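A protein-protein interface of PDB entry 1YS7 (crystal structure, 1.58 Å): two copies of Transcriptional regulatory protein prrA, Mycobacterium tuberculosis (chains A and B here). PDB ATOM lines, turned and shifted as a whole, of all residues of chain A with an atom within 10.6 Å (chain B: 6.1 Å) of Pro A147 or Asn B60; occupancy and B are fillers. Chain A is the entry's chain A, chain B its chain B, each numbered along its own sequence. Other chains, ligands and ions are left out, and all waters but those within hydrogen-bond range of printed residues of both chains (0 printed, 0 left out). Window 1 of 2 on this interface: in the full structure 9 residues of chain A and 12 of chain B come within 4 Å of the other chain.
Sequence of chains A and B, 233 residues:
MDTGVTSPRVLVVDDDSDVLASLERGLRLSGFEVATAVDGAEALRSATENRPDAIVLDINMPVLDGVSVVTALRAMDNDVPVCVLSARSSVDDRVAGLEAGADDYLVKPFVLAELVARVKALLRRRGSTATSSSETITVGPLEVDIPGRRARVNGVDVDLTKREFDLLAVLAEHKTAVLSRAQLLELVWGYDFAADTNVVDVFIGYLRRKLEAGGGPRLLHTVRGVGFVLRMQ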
ATOM      1  N   ASP A  79      26.084  29.641  -0.407  1.00  0.00           N
ATOM      2  CA  ASP A  79      26.270  28.486   0.442  1.00  0.00           C
ATOM      3  C   ASP A  79      27.058  28.780   1.716  1.00  0.00           C
ATOM      4  O   ASP A  79      27.528  27.847   2.383  1.00  0.00           O
ATOM      5  CB  ASP A  79      26.870  27.312  -0.327  1.00  0.00           C
ATOM      6  CG  ASP A  79      25.846  26.636  -1.244  1.00  0.00           C
ATOM      7  OD1 ASP A  79      24.623  26.634  -0.961  1.00  0.00           O
ATOM      8  OD2 ASP A  79      26.285  26.111  -2.278  1.00  0.00           O
ATOM      9  N   THR A 129      38.938  20.753   1.162  1.00  0.00           N
ATOM     10  CA  THR A 129      39.068  20.597  -0.269  1.00  0.00           C
ATOM     11  C   THR A 129      39.110  19.118  -0.677  1.00  0.00           C
ATOM     12  O   THR A 129      39.317  18.833  -1.858  1.00  0.00           O
ATOM     13  CB  THR A 129      40.297  21.348  -0.838  1.00  0.00           C
ATOM     14  OG1 THR A 129      41.493  20.761  -0.328  1.00  0.00           O
ATOM     15  CG2 THR A 129      40.255  22.851  -0.488  1.00  0.00           C
ATOM     16  N   ALA A 130      38.864  18.208   0.269  1.00  0.00           N
ATOM     17  CA  ALA A 130      38.869  16.770   0.008  1.00  0.00           C
ATOM     18  C   ALA A 130      37.846  16.458  -1.081  1.00  0.00           C
ATOM     19  O   ALA A 130      36.664  16.841  -0.950  1.00  0.00           O
ATOM     20  CB  ALA A 130      38.502  15.988   1.276  1.00  0.00           C
ATOM     21  N   THR A 131      38.274  15.797  -2.167  1.00  0.00           N
ATOM     22  CA  THR A 131      37.314  15.396  -3.213  1.00  0.00           C
ATOM     23  C   THR A 131      37.326  13.905  -3.543  1.00  0.00           C
ATOM     24  O   THR A 131      38.366  13.274  -3.770  1.00  0.00           O
ATOM     25  CB  THR A 131      37.224  16.354  -4.479  1.00  0.00           C
ATOM     26  OG1 THR A 131      37.667  15.716  -5.678  1.00  0.00           O
ATOM     27  CG2 THR A 131      37.949  17.648  -4.266  1.00  0.00           C
ATOM     28  N   SER A 132      36.130  13.354  -3.511  1.00  0.00           N
ATOM     29  CA  SER A 132      35.884  11.954  -3.713  1.00  0.00           C
ATOM     30  C   SER A 132      36.089  11.567  -5.179  1.00  0.00           C
ATOM     31  O   SER A 132      35.954  12.409  -6.051  1.00  0.00           O
ATOM     32  CB  SER A 132      34.412  11.734  -3.358  1.00  0.00           C
ATOM     33  OG  SER A 132      33.966  10.568  -3.957  1.00  0.00           O
ATOM     34  N   SER A 133      36.373  10.291  -5.432  1.00  0.00           N
ATOM     35  CA  SER A 133      36.399   9.791  -6.798  1.00  0.00           C
ATOM     36  C   SER A 133      34.994   9.396  -7.294  1.00  0.00           C
ATOM     37  O   SER A 133      34.806   9.103  -8.494  1.00  0.00           O
ATOM     38  CB  SER A 133      37.357   8.592  -6.937  1.00  0.00           C
ATOM     39  OG  SER A 133      36.907   7.558  -6.071  1.00  0.00           O
ATOM     40  N   SER A 134      34.009   9.444  -6.387  1.00  0.00           N
ATOM     41  CA  SER A 134      32.676   8.968  -6.731  1.00  0.00           C
ATOM     42  C   SER A 134      31.971   9.857  -7.759  1.00  0.00           C
ATOM     43  O   SER A 134      32.079  11.101  -7.736  1.00  0.00           O
ATOM     44  CB  SER A 134      31.820   8.831  -5.472  1.00  0.00           C
ATOM     45  OG  SER A 134      32.427   7.897  -4.587  1.00  0.00           O
ATOM     46  N   GLU A 135      31.219   9.215  -8.660  1.00  0.00           N
ATOM     47  CA  GLU A 135      30.428   9.877  -9.673  1.00  0.00           C
ATOM     48  C   GLU A 135      28.952   9.790  -9.246  1.00  0.00           C
ATOM     49  O   GLU A 135      28.571  10.414  -8.245  1.00  0.00           O
ATOM     50  CB  GLU A 135      30.742   9.193 -11.021  1.00  0.00           C
ATOM     51  CG  GLU A 135      32.319   9.148 -11.238  1.00  0.00           C
ATOM     52  CD  GLU A 135      32.760   8.402 -12.510  1.00  0.00           C
ATOM     53  OE1 GLU A 135      33.989   8.286 -12.722  1.00  0.00           O
ATOM     54  OE2 GLU A 135      31.883   7.926 -13.274  1.00  0.00           O
ATOM     55  N   THR A 136      28.139   9.022  -9.967  1.00  0.00           N
ATOM     56  CA  THR A 136      26.742   8.877  -9.557  1.00  0.00           C
ATOM     57  C   THR A 136      26.607   7.557  -8.859  1.00  0.00           C
ATOM     58  O   THR A 136      26.931   6.538  -9.411  1.00  0.00           O
ATOM     59  CB  THR A 136      25.755   8.945 -10.730  1.00  0.00           C
ATOM     60  OG1 THR A 136      25.840  10.238 -11.347  1.00  0.00           O
ATOM     61  CG2 THR A 136      24.287   8.722 -10.248  1.00  0.00           C
ATOM     62  N   ILE A 137      26.101   7.579  -7.621  1.00  0.00           N
ATOM     63  CA  ILE A 137      26.011   6.380  -6.770  1.00  0.00           C
ATOM     64  C   ILE A 137      24.551   5.956  -6.776  1.00  0.00           C
ATOM     65  O   ILE A 137      23.668   6.772  -6.614  1.00  0.00           O
ATOM     66  CB  ILE A 137      26.476   6.690  -5.318  1.00  0.00           C
ATOM     67  CG1 ILE A 137      27.982   7.030  -5.328  1.00  0.00           C
ATOM     68  CG2 ILE A 137      26.222   5.469  -4.353  1.00  0.00           C
ATOM     69  CD1 ILE A 137      28.526   7.604  -4.018  1.00  0.00           C
ATOM     70  N   GLU A 143      19.442   7.778  -7.015  1.00  0.00           N
ATOM     71  CA  GLU A 143      20.707   8.066  -7.694  1.00  0.00           C
ATOM     72  C   GLU A 143      21.230   9.323  -7.024  1.00  0.00           C
ATOM     73  O   GLU A 143      20.500  10.316  -6.979  1.00  0.00           O
ATOM     74  CB  GLU A 143      20.455   8.333  -9.169  1.00  0.00           C
ATOM     75  CG  GLU A 143      20.320   7.058  -9.984  1.00  0.00           C
ATOM     76  CD  GLU A 143      20.476   7.320 -11.467  1.00  0.00           C
ATOM     77  OE1 GLU A 143      20.422   8.503 -11.891  1.00  0.00           O
ATOM     78  OE2 GLU A 143      20.678   6.339 -12.201  1.00  0.00           O
ATOM     79  N   VAL A 144      22.471   9.294  -6.563  1.00  0.00           N
ATOM     80  CA  VAL A 144      23.164  10.464  -5.979  1.00  0.00           C
ATOM     81  C   VAL A 144      24.339  10.844  -6.894  1.00  0.00           C
ATOM     82  O   VAL A 144      25.336  10.116  -6.929  1.00  0.00           O
ATOM     83  CB  VAL A 144      23.658  10.163  -4.538  1.00  0.00           C
ATOM     84  CG1 VAL A 144      24.284  11.431  -3.932  1.00  0.00           C
ATOM     85  CG2 VAL A 144      22.486   9.732  -3.737  1.00  0.00           C
ATOM     86  N   ASP A 145      24.183  11.976  -7.569  1.00  0.00           N
ATOM     87  CA  ASP A 145      25.254  12.536  -8.398  1.00  0.00           C
ATOM     88  C   ASP A 145      26.123  13.365  -7.441  1.00  0.00           C
ATOM     89  O   ASP A 145      25.739  14.491  -7.067  1.00  0.00           O
ATOM     90  CB  ASP A 145      24.653  13.402  -9.498  1.00  0.00           C
ATOM     91  CG  ASP A 145      25.719  14.190 -10.279  1.00  0.00           C
ATOM     92  OD1 ASP A 145      26.914  14.052  -9.964  1.00  0.00           O
ATOM     93  OD2 ASP A 145      25.287  14.977 -11.153  1.00  0.00           O
ATOM     94  N   ILE A 146      27.287  12.833  -7.046  1.00  0.00           N
ATOM     95  CA  ILE A 146      28.117  13.449  -5.966  1.00  0.00           C
ATOM     96  C   ILE A 146      28.678  14.816  -6.481  1.00  0.00           C
ATOM     97  O   ILE A 146      28.378  15.873  -5.897  1.00  0.00           O
ATOM     98  CB  ILE A 146      29.198  12.468  -5.481  1.00  0.00           C
ATOM     99  CG1 ILE A 146      28.528  11.306  -4.731  1.00  0.00           C
ATOM    100  CG2 ILE A 146      30.217  13.175  -4.573  1.00  0.00           C
ATOM    101  CD1 ILE A 146      27.880  11.761  -3.469  1.00  0.00           C
ATOM    102  N   PRO A 147      29.466  14.812  -7.589  1.00  0.00           N
ATOM    103  CA  PRO A 147      30.014  16.101  -8.016  1.00  0.00           C
ATOM    104  C   PRO A 147      28.961  17.112  -8.434  1.00  0.00           C
ATOM    105  O   PRO A 147      29.137  18.323  -8.149  1.00  0.00           O
ATOM    106  CB  PRO A 147      30.895  15.738  -9.224  1.00  0.00           C
ATOM    107  CG  PRO A 147      30.311  14.474  -9.719  1.00  0.00           C
ATOM    108  CD  PRO A 147      29.901  13.719  -8.448  1.00  0.00           C
ATOM    109  N   GLY A 148      27.870  16.651  -9.050  1.00  0.00           N
ATOM    110  CA  GLY A 148      26.761  17.498  -9.440  1.00  0.00           C
ATOM    111  C   GLY A 148      25.811  17.917  -8.319  1.00  0.00           C
ATOM    112  O   GLY A 148      24.973  18.792  -8.519  1.00  0.00           O
ATOM    113  N   ARG A 149      25.981  17.316  -7.146  1.00  0.00           N
ATOM    114  CA  ARG A 149      25.139  17.674  -5.994  1.00  0.00           C
ATOM    115  C   ARG A 149      23.634  17.602  -6.288  1.00  0.00           C
ATOM    116  O   ARG A 149      22.850  18.512  -5.923  1.00  0.00           O
ATOM    117  CB  ARG A 149      25.582  19.034  -5.410  1.00  0.00           C
ATOM    118  CG  ARG A 149      26.974  18.931  -4.778  1.00  0.00           C
ATOM    119  CD  ARG A 149      27.412  20.183  -4.028  1.00  0.00           C
ATOM    120  NE  ARG A 149      26.514  20.431  -2.906  1.00  0.00           N
ATOM    121  CZ  ARG A 149      26.718  19.974  -1.678  1.00  0.00           C
ATOM    122  NH1 ARG A 149      27.782  19.232  -1.402  1.00  0.00           N
ATOM    123  NH2 ARG A 149      25.823  20.257  -0.724  1.00  0.00           N
ATOM    124  N   ARG A 150      23.226  16.514  -6.951  1.00  0.00           N
ATOM    125  CA  ARG A 150      21.827  16.244  -7.208  1.00  0.00           C
ATOM    126  C   ARG A 150      21.489  14.819  -6.801  1.00  0.00           C
ATOM    127  O   ARG A 150      22.329  13.918  -6.832  1.00  0.00           O
ATOM    128  CB  ARG A 150      21.470  16.493  -8.684  1.00  0.00           C
ATOM    129  CG  ARG A 150      21.686  15.342  -9.636  1.00  0.00           C
ATOM    130  CD  ARG A 150      20.356  14.777 -10.265  1.00  0.00           C
ATOM    131  NE  ARG A 150      20.564  13.718 -11.279  1.00  0.00           N
ATOM    132  CZ  ARG A 150      20.745  12.428 -10.999  1.00  0.00           C
ATOM    133  NH1 ARG A 150      20.948  11.548 -11.968  1.00  0.00           N
ATOM    134  NH2 ARG A 150      20.756  12.014  -9.736  1.00  0.00           N
ATOM    135  N   ALA A 151      20.255  14.664  -6.343  1.00  0.00           N
ATOM    136  CA  ALA A 151      19.712  13.372  -6.021  1.00  0.00           C
ATOM    137  C   ALA A 151      18.367  13.191  -6.692  1.00  0.00           C
ATOM    138  O   ALA A 151      17.568  14.126  -6.750  1.00  0.00           O
ATOM    139  CB  ALA A 151      19.547  13.250  -4.508  1.00  0.00           C
ATOM    140  N   PHE A 165      22.173  17.430   1.644  1.00  0.00           N
ATOM    141  CA  PHE A 165      22.888  16.722   0.597  1.00  0.00           C
ATOM    142  C   PHE A 165      24.277  16.267   1.075  1.00  0.00           C
ATOM    143  O   PHE A 165      24.751  15.164   0.727  1.00  0.00           O
ATOM    144  CB  PHE A 165      23.049  17.571  -0.685  1.00  0.00           C
ATOM    145  CG  PHE A 165      23.679  16.781  -1.792  1.00  0.00           C
ATOM    146  CD1 PHE A 165      22.888  16.058  -2.671  1.00  0.00           C
ATOM    147  CD2 PHE A 165      25.074  16.667  -1.884  1.00  0.00           C
ATOM    148  CE1 PHE A 165      23.515  15.245  -3.624  1.00  0.00           C
ATOM    149  CE2 PHE A 165      25.666  15.890  -2.853  1.00  0.00           C
ATOM    150  CZ  PHE A 165      24.901  15.208  -3.701  1.00  0.00           C
ATOM    151  N   ASP A 166      24.948  17.103   1.863  1.00  0.00           N
ATOM    152  CA  ASP A 166      26.285  16.739   2.433  1.00  0.00           C
ATOM    153  C   ASP A 166      26.142  15.423   3.208  1.00  0.00           C
ATOM    154  O   ASP A 166      26.951  14.494   3.105  1.00  0.00           O
ATOM    155  CB  ASP A 166      26.821  17.770   3.447  1.00  0.00           C
ATOM    156  CG  ASP A 166      27.219  19.107   2.811  1.00  0.00           C
ATOM    157  OD1 ASP A 166      27.446  19.107   1.584  1.00  0.00           O
ATOM    158  OD2 ASP A 166      27.300  20.131   3.575  1.00  0.00           O
ATOM    159  N   ALA A 169      25.350  12.561   0.844  1.00  0.00           N
ATOM    160  CA  ALA A 169      26.553  12.262   0.063  1.00  0.00           C
ATOM    161  C   ALA A 169      27.507  11.336   0.809  1.00  0.00           C
ATOM    162  O   ALA A 169      27.994  10.339   0.253  1.00  0.00           O
ATOM    163  CB  ALA A 169      27.247  13.525  -0.354  1.00  0.00           C
ATOM    164  N   VAL A 170      27.769  11.634   2.074  1.00  0.00           N
ATOM    165  CA  VAL A 170      28.676  10.795   2.907  1.00  0.00           C
ATOM    166  C   VAL A 170      28.080   9.393   3.041  1.00  0.00           C
ATOM    167  O   VAL A 170      28.768   8.353   2.931  1.00  0.00           O
ATOM    168  CB  VAL A 170      28.968  11.461   4.229  1.00  0.00           C
ATOM    169  CG1 VAL A 170      29.707  10.532   5.144  1.00  0.00           C
ATOM    170  CG2 VAL A 170      29.745  12.794   3.988  1.00  0.00           C
ATOM    171  N   ALA A 172      26.145   7.868   1.053  1.00  0.00           N
ATOM    172  CA  ALA A 172      26.169   7.191  -0.233  1.00  0.00           C
ATOM    173  C   ALA A 172      27.616   6.806  -0.614  1.00  0.00           C
ATOM    174  O   ALA A 172      27.800   5.716  -1.141  1.00  0.00           O
ATOM    175  CB  ALA A 172      25.587   8.060  -1.300  1.00  0.00           C
ATOM    176  N   GLU A 173      28.593   7.667  -0.319  1.00  0.00           N
ATOM    177  CA  GLU A 173      30.020   7.360  -0.500  1.00  0.00           C
ATOM    178  C   GLU A 173      30.386   6.080   0.255  1.00  0.00           C
ATOM    179  O   GLU A 173      31.247   5.309  -0.150  1.00  0.00           O
ATOM    180  CB  GLU A 173      30.846   8.537   0.050  1.00  0.00           C
ATOM    181  CG  GLU A 173      30.829   9.716  -0.862  1.00  0.00           C
ATOM    182  CD  GLU A 173      31.724   9.585  -2.017  1.00  0.00           C
ATOM    183  OE1 GLU A 173      32.232   8.460  -2.263  1.00  0.00           O
ATOM    184  OE2 GLU A 173      31.946  10.630  -2.679  1.00  0.00           O
ATOM    185  N   ASP B  14      35.264  17.632 -18.673  1.00  0.00           N
ATOM    186  CA  ASP B  14      33.920  17.589 -18.018  1.00  0.00           C
ATOM    187  C   ASP B  14      33.658  16.151 -17.661  1.00  0.00           C
ATOM    188  O   ASP B  14      34.013  15.239 -18.445  1.00  0.00           O
ATOM    189  CB  ASP B  14      32.847  18.175 -18.976  1.00  0.00           C
ATOM    190  CG  ASP B  14      31.572  18.556 -18.275  1.00  0.00           C
ATOM    191  OD1 ASP B  14      30.964  17.692 -17.626  1.00  0.00           O
ATOM    192  OD2 ASP B  14      31.186  19.739 -18.354  1.00  0.00           O
ATOM    193  N   ASP B  15      33.078  15.935 -16.480  1.00  0.00           N
ATOM    194  CA  ASP B  15      32.723  14.593 -16.050  1.00  0.00           C
ATOM    195  C   ASP B  15      31.368  14.097 -16.562  1.00  0.00           C
ATOM    196  O   ASP B  15      31.028  12.921 -16.305  1.00  0.00           O
ATOM    197  CB  ASP B  15      32.820  14.516 -14.536  1.00  0.00           C
ATOM    198  CG  ASP B  15      31.829  15.433 -13.859  1.00  0.00           C
ATOM    199  OD1 ASP B  15      31.660  16.604 -14.268  1.00  0.00           O
ATOM    200  OD2 ASP B  15      31.163  14.918 -12.940  1.00  0.00           O
ATOM    201  N   ASP B  58      35.225  22.195 -16.631  1.00  0.00           N
ATOM    202  CA  ASP B  58      34.076  22.062 -15.725  1.00  0.00           C
ATOM    203  C   ASP B  58      34.581  22.177 -14.277  1.00  0.00           C
ATOM    204  O   ASP B  58      35.669  21.706 -13.904  1.00  0.00           O
ATOM    205  CB  ASP B  58      33.412  20.737 -16.001  1.00  0.00           C
ATOM    206  CG  ASP B  58      32.197  20.467 -15.100  1.00  0.00           C
ATOM    207  OD1 ASP B  58      31.402  21.410 -14.935  1.00  0.00           O
ATOM    208  OD2 ASP B  58      32.009  19.295 -14.649  1.00  0.00           O
ATOM    209  N   ILE B  59      33.798  22.879 -13.448  1.00  0.00           N
ATOM    210  CA  ILE B  59      34.244  23.049 -12.059  1.00  0.00           C
ATOM    211  C   ILE B  59      33.983  21.804 -11.190  1.00  0.00           C
ATOM    212  O   ILE B  59      34.869  21.336 -10.459  1.00  0.00           O
ATOM    213  CB  ILE B  59      33.566  24.228 -11.411  1.00  0.00           C
ATOM    214  CG1 ILE B  59      34.017  25.501 -12.103  1.00  0.00           C
ATOM    215  CG2 ILE B  59      33.916  24.275  -9.896  1.00  0.00           C
ATOM    216  CD1 ILE B  59      35.431  25.888 -11.742  1.00  0.00           C
ATOM    217  N   ASN B  60      32.758  21.289 -11.268  1.00  0.00           N
ATOM    218  CA  ASN B  60      32.365  20.193 -10.411  1.00  0.00           C
ATOM    219  C   ASN B  60      32.587  18.861 -11.078  1.00  0.00           C
ATOM    220  O   ASN B  60      31.805  18.442 -11.970  1.00  0.00           O
ATOM    221  CB  ASN B  60      30.925  20.408 -10.063  1.00  0.00           C
ATOM    222  CG  ASN B  60      30.754  21.654  -9.227  1.00  0.00           C
ATOM    223  OD1 ASN B  60      31.437  21.808  -8.210  1.00  0.00           O
ATOM    224  ND2 ASN B  60      29.920  22.571  -9.674  1.00  0.00           N
ATOM    225  N   MET B  61      33.621  18.201 -10.576  1.00  0.00           N
ATOM    226  CA  MET B  61      34.079  16.886 -11.081  1.00  0.00           C
ATOM    227  C   MET B  61      34.627  16.039 -10.004  1.00  0.00           C
ATOM    228  O   MET B  61      35.053  16.590  -8.983  1.00  0.00           O
ATOM    229  CB  MET B  61      35.224  17.123 -12.058  1.00  0.00           C
ATOM    230  CG  MET B  61      34.874  17.971 -13.235  1.00  0.00           C
ATOM    231  SD  MET B  61      36.293  18.013 -14.399  1.00  0.00           S
ATOM    232  CE  MET B  61      37.459  19.051 -13.579  1.00  0.00           C
ATOM    233  N   PRO B  62      34.701  14.709 -10.216  1.00  0.00           N
ATOM    234  CA  PRO B  62      35.280  13.852  -9.174  1.00  0.00           C
ATOM    235  C   PRO B  62      36.784  13.848  -9.245  1.00  0.00           C
ATOM    236  O   PRO B  62      37.323  14.370 -10.235  1.00  0.00           O
ATOM    237  CB  PRO B  62      34.775  12.450  -9.543  1.00  0.00           C
ATOM    238  CG  PRO B  62      34.552  12.503 -11.000  1.00  0.00           C
ATOM    239  CD  PRO B  62      34.206  13.929 -11.374  1.00  0.00           C
ATOM    240  N   ASP B  65      38.658  18.506  -8.645  1.00  0.00           N
ATOM    241  CA  ASP B  65      37.698  19.427  -9.223  1.00  0.00           C
ATOM    242  C   ASP B  65      38.358  20.582  -9.984  1.00  0.00           C
ATOM    243  O   ASP B  65      39.618  20.676  -9.979  1.00  0.00           O
ATOM    244  CB  ASP B  65      36.622  19.906  -8.200  1.00  0.00           C
ATOM    245  CG  ASP B  65      37.169  20.848  -7.108  1.00  0.00           C
ATOM    246  OD1 ASP B  65      38.190  21.533  -7.264  1.00  0.00           O
ATOM    247  OD2 ASP B  65      36.542  20.976  -6.010  1.00  0.00           O
ATOM    248  N   GLY B  66      37.537  21.398 -10.659  1.00  0.00           N
ATOM    249  CA  GLY B  66      38.098  22.476 -11.543  1.00  0.00           C
ATOM    250  C   GLY B  66      38.839  23.510 -10.725  1.00  0.00           C
ATOM    251  O   GLY B  66      39.847  24.051 -11.181  1.00  0.00           O
ATOM    252  N   LEU B  85      33.439  26.180 -16.646  1.00  0.00           N
ATOM    253  CA  LEU B  85      31.995  25.952 -16.839  1.00  0.00           C
ATOM    254  C   LEU B  85      31.355  25.558 -15.534  1.00  0.00           C
ATOM    255  O   LEU B  85      31.929  24.819 -14.733  1.00  0.00           O
ATOM    256  CB  LEU B  85      31.755  24.794 -17.778  1.00  0.00           C
ATOM    257  CG  LEU B  85      32.520  24.777 -19.114  1.00  0.00           C
ATOM    258  CD1 LEU B  85      32.163  23.520 -19.845  1.00  0.00           C
ATOM    259  CD2 LEU B  85      32.096  25.994 -19.893  1.00  0.00           C
ATOM    260  N   SER B  86      30.115  25.991 -15.360  1.00  0.00           N
ATOM    261  CA  SER B  86      29.351  25.510 -14.207  1.00  0.00           C
ATOM    262  C   SER B  86      27.870  25.654 -14.442  1.00  0.00           C
ATOM    263  O   SER B  86      27.476  26.424 -15.286  1.00  0.00           O
ATOM    264  CB  SER B  86      29.734  26.288 -12.951  1.00  0.00           C
ATOM    265  OG  SER B  86      29.407  27.658 -13.050  1.00  0.00           O
ATOM    266  N   ALA B  87      27.057  24.928 -13.661  1.00  0.00           N
ATOM    267  CA  ALA B  87      25.598  25.061 -13.702  1.00  0.00           C
ATOM    268  C   ALA B  87      25.215  26.412 -13.185  1.00  0.00           C
ATOM    269  O   ALA B  87      25.937  26.959 -12.371  1.00  0.00           O
ATOM    270  CB  ALA B  87      24.957  23.977 -12.831  1.00  0.00           C
ATOM    271  N   SER B  90      25.412  27.092  -9.459  1.00  0.00           N
ATOM    272  CA  SER B  90      26.640  26.854  -8.742  1.00  0.00           C
ATOM    273  C   SER B  90      27.521  28.121  -8.734  1.00  0.00           C
ATOM    274  O   SER B  90      28.671  28.115  -9.206  1.00  0.00           O
ATOM    275  CB  SER B  90      27.365  25.671  -9.366  1.00  0.00           C
ATOM    276  OG  SER B  90      26.459  24.568  -9.513  1.00  0.00           O
ATOM    277  N   ASP B  93      30.993  28.134  -6.740  1.00  0.00           N
ATOM    278  CA  ASP B  93      31.978  27.275  -7.384  1.00  0.00           C
ATOM    279  C   ASP B  93      32.683  27.997  -8.510  1.00  0.00           C
ATOM    280  O   ASP B  93      33.926  27.955  -8.573  1.00  0.00           O
ATOM    281  CB  ASP B  93      31.256  26.071  -8.001  1.00  0.00           C
ATOM    282  CG  ASP B  93      30.662  25.145  -6.956  1.00  0.00           C
ATOM    283  OD1 ASP B  93      29.456  24.809  -7.084  1.00  0.00           O
ATOM    284  OD2 ASP B  93      31.393  24.774  -6.009  1.00  0.00           O
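The backbone NH of Ser A134 sits at hydrogen-bond distance from the side-chain hydroxyl of Ser A132. OE1 of Glu A173 sits close to OG of Ser A132, 3.2 Å away. OG of Ser A134 sits close to OE2 of Glu A173 (3.4 Å). OD1 of Asp B93 lies within hydrogen-bond range of ND2 of Asn B60 (3.5 Å).
Among the printed residues, pairs that only touch across the chains: Ser A132 with Pro B62 (3.5 Å), Ser A133 with Pro B62 (3.5 Å), Ser A134 with Pro B62 (3.5 Å), Pro A147 with Asp B15 (3.4 Å), Pro A147 with Asn B60 (3.3 Å) and Pro A147 with Met B61 (3.8 Å).
No position is printed for both chains. Of the 6 pairs that touch across the chains among the printed residues, none has its exchanged pair printed and touching as well.
Printed residues of chain B within 4 Å of Ser A134: Pro B62 (3.5 Å). Of chain B, only Asp B15, Asn B60 and Met B61 come within 4 Å of Pro A147. Of the printed residues of chain A, Asp B15 touches Pro A147 (3.4 Å). No residue of chain A comes within 4 Å of Asp B58. No residue of chain A comes within 4 Å of Ile B59. Asn B60 touches just one residue of chain A: Pro A147 (3.3 Å). Of chain A, only Pro A147 (3.8 Å) comes within 4 Å of Met B61. No residue of chain A comes within 4 Å of Ser B90. The nearest printed residue of chain A that does not touch Pro B62 is Glu A135 (4.04 Å).
Of the 14 printed residues of chain B, 4 touch a printed residue of chain A. Hydrophobic or aromatic side chains of chain A within 4 Å of the printed part of chain B: Pro A147. Among the printed residues, 6 pairs touch across the chains. Among the printed residues, no Asp or Glu carboxylate lies within 4 Å of a Lys or Arg side-chain nitrogen of the other chain.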
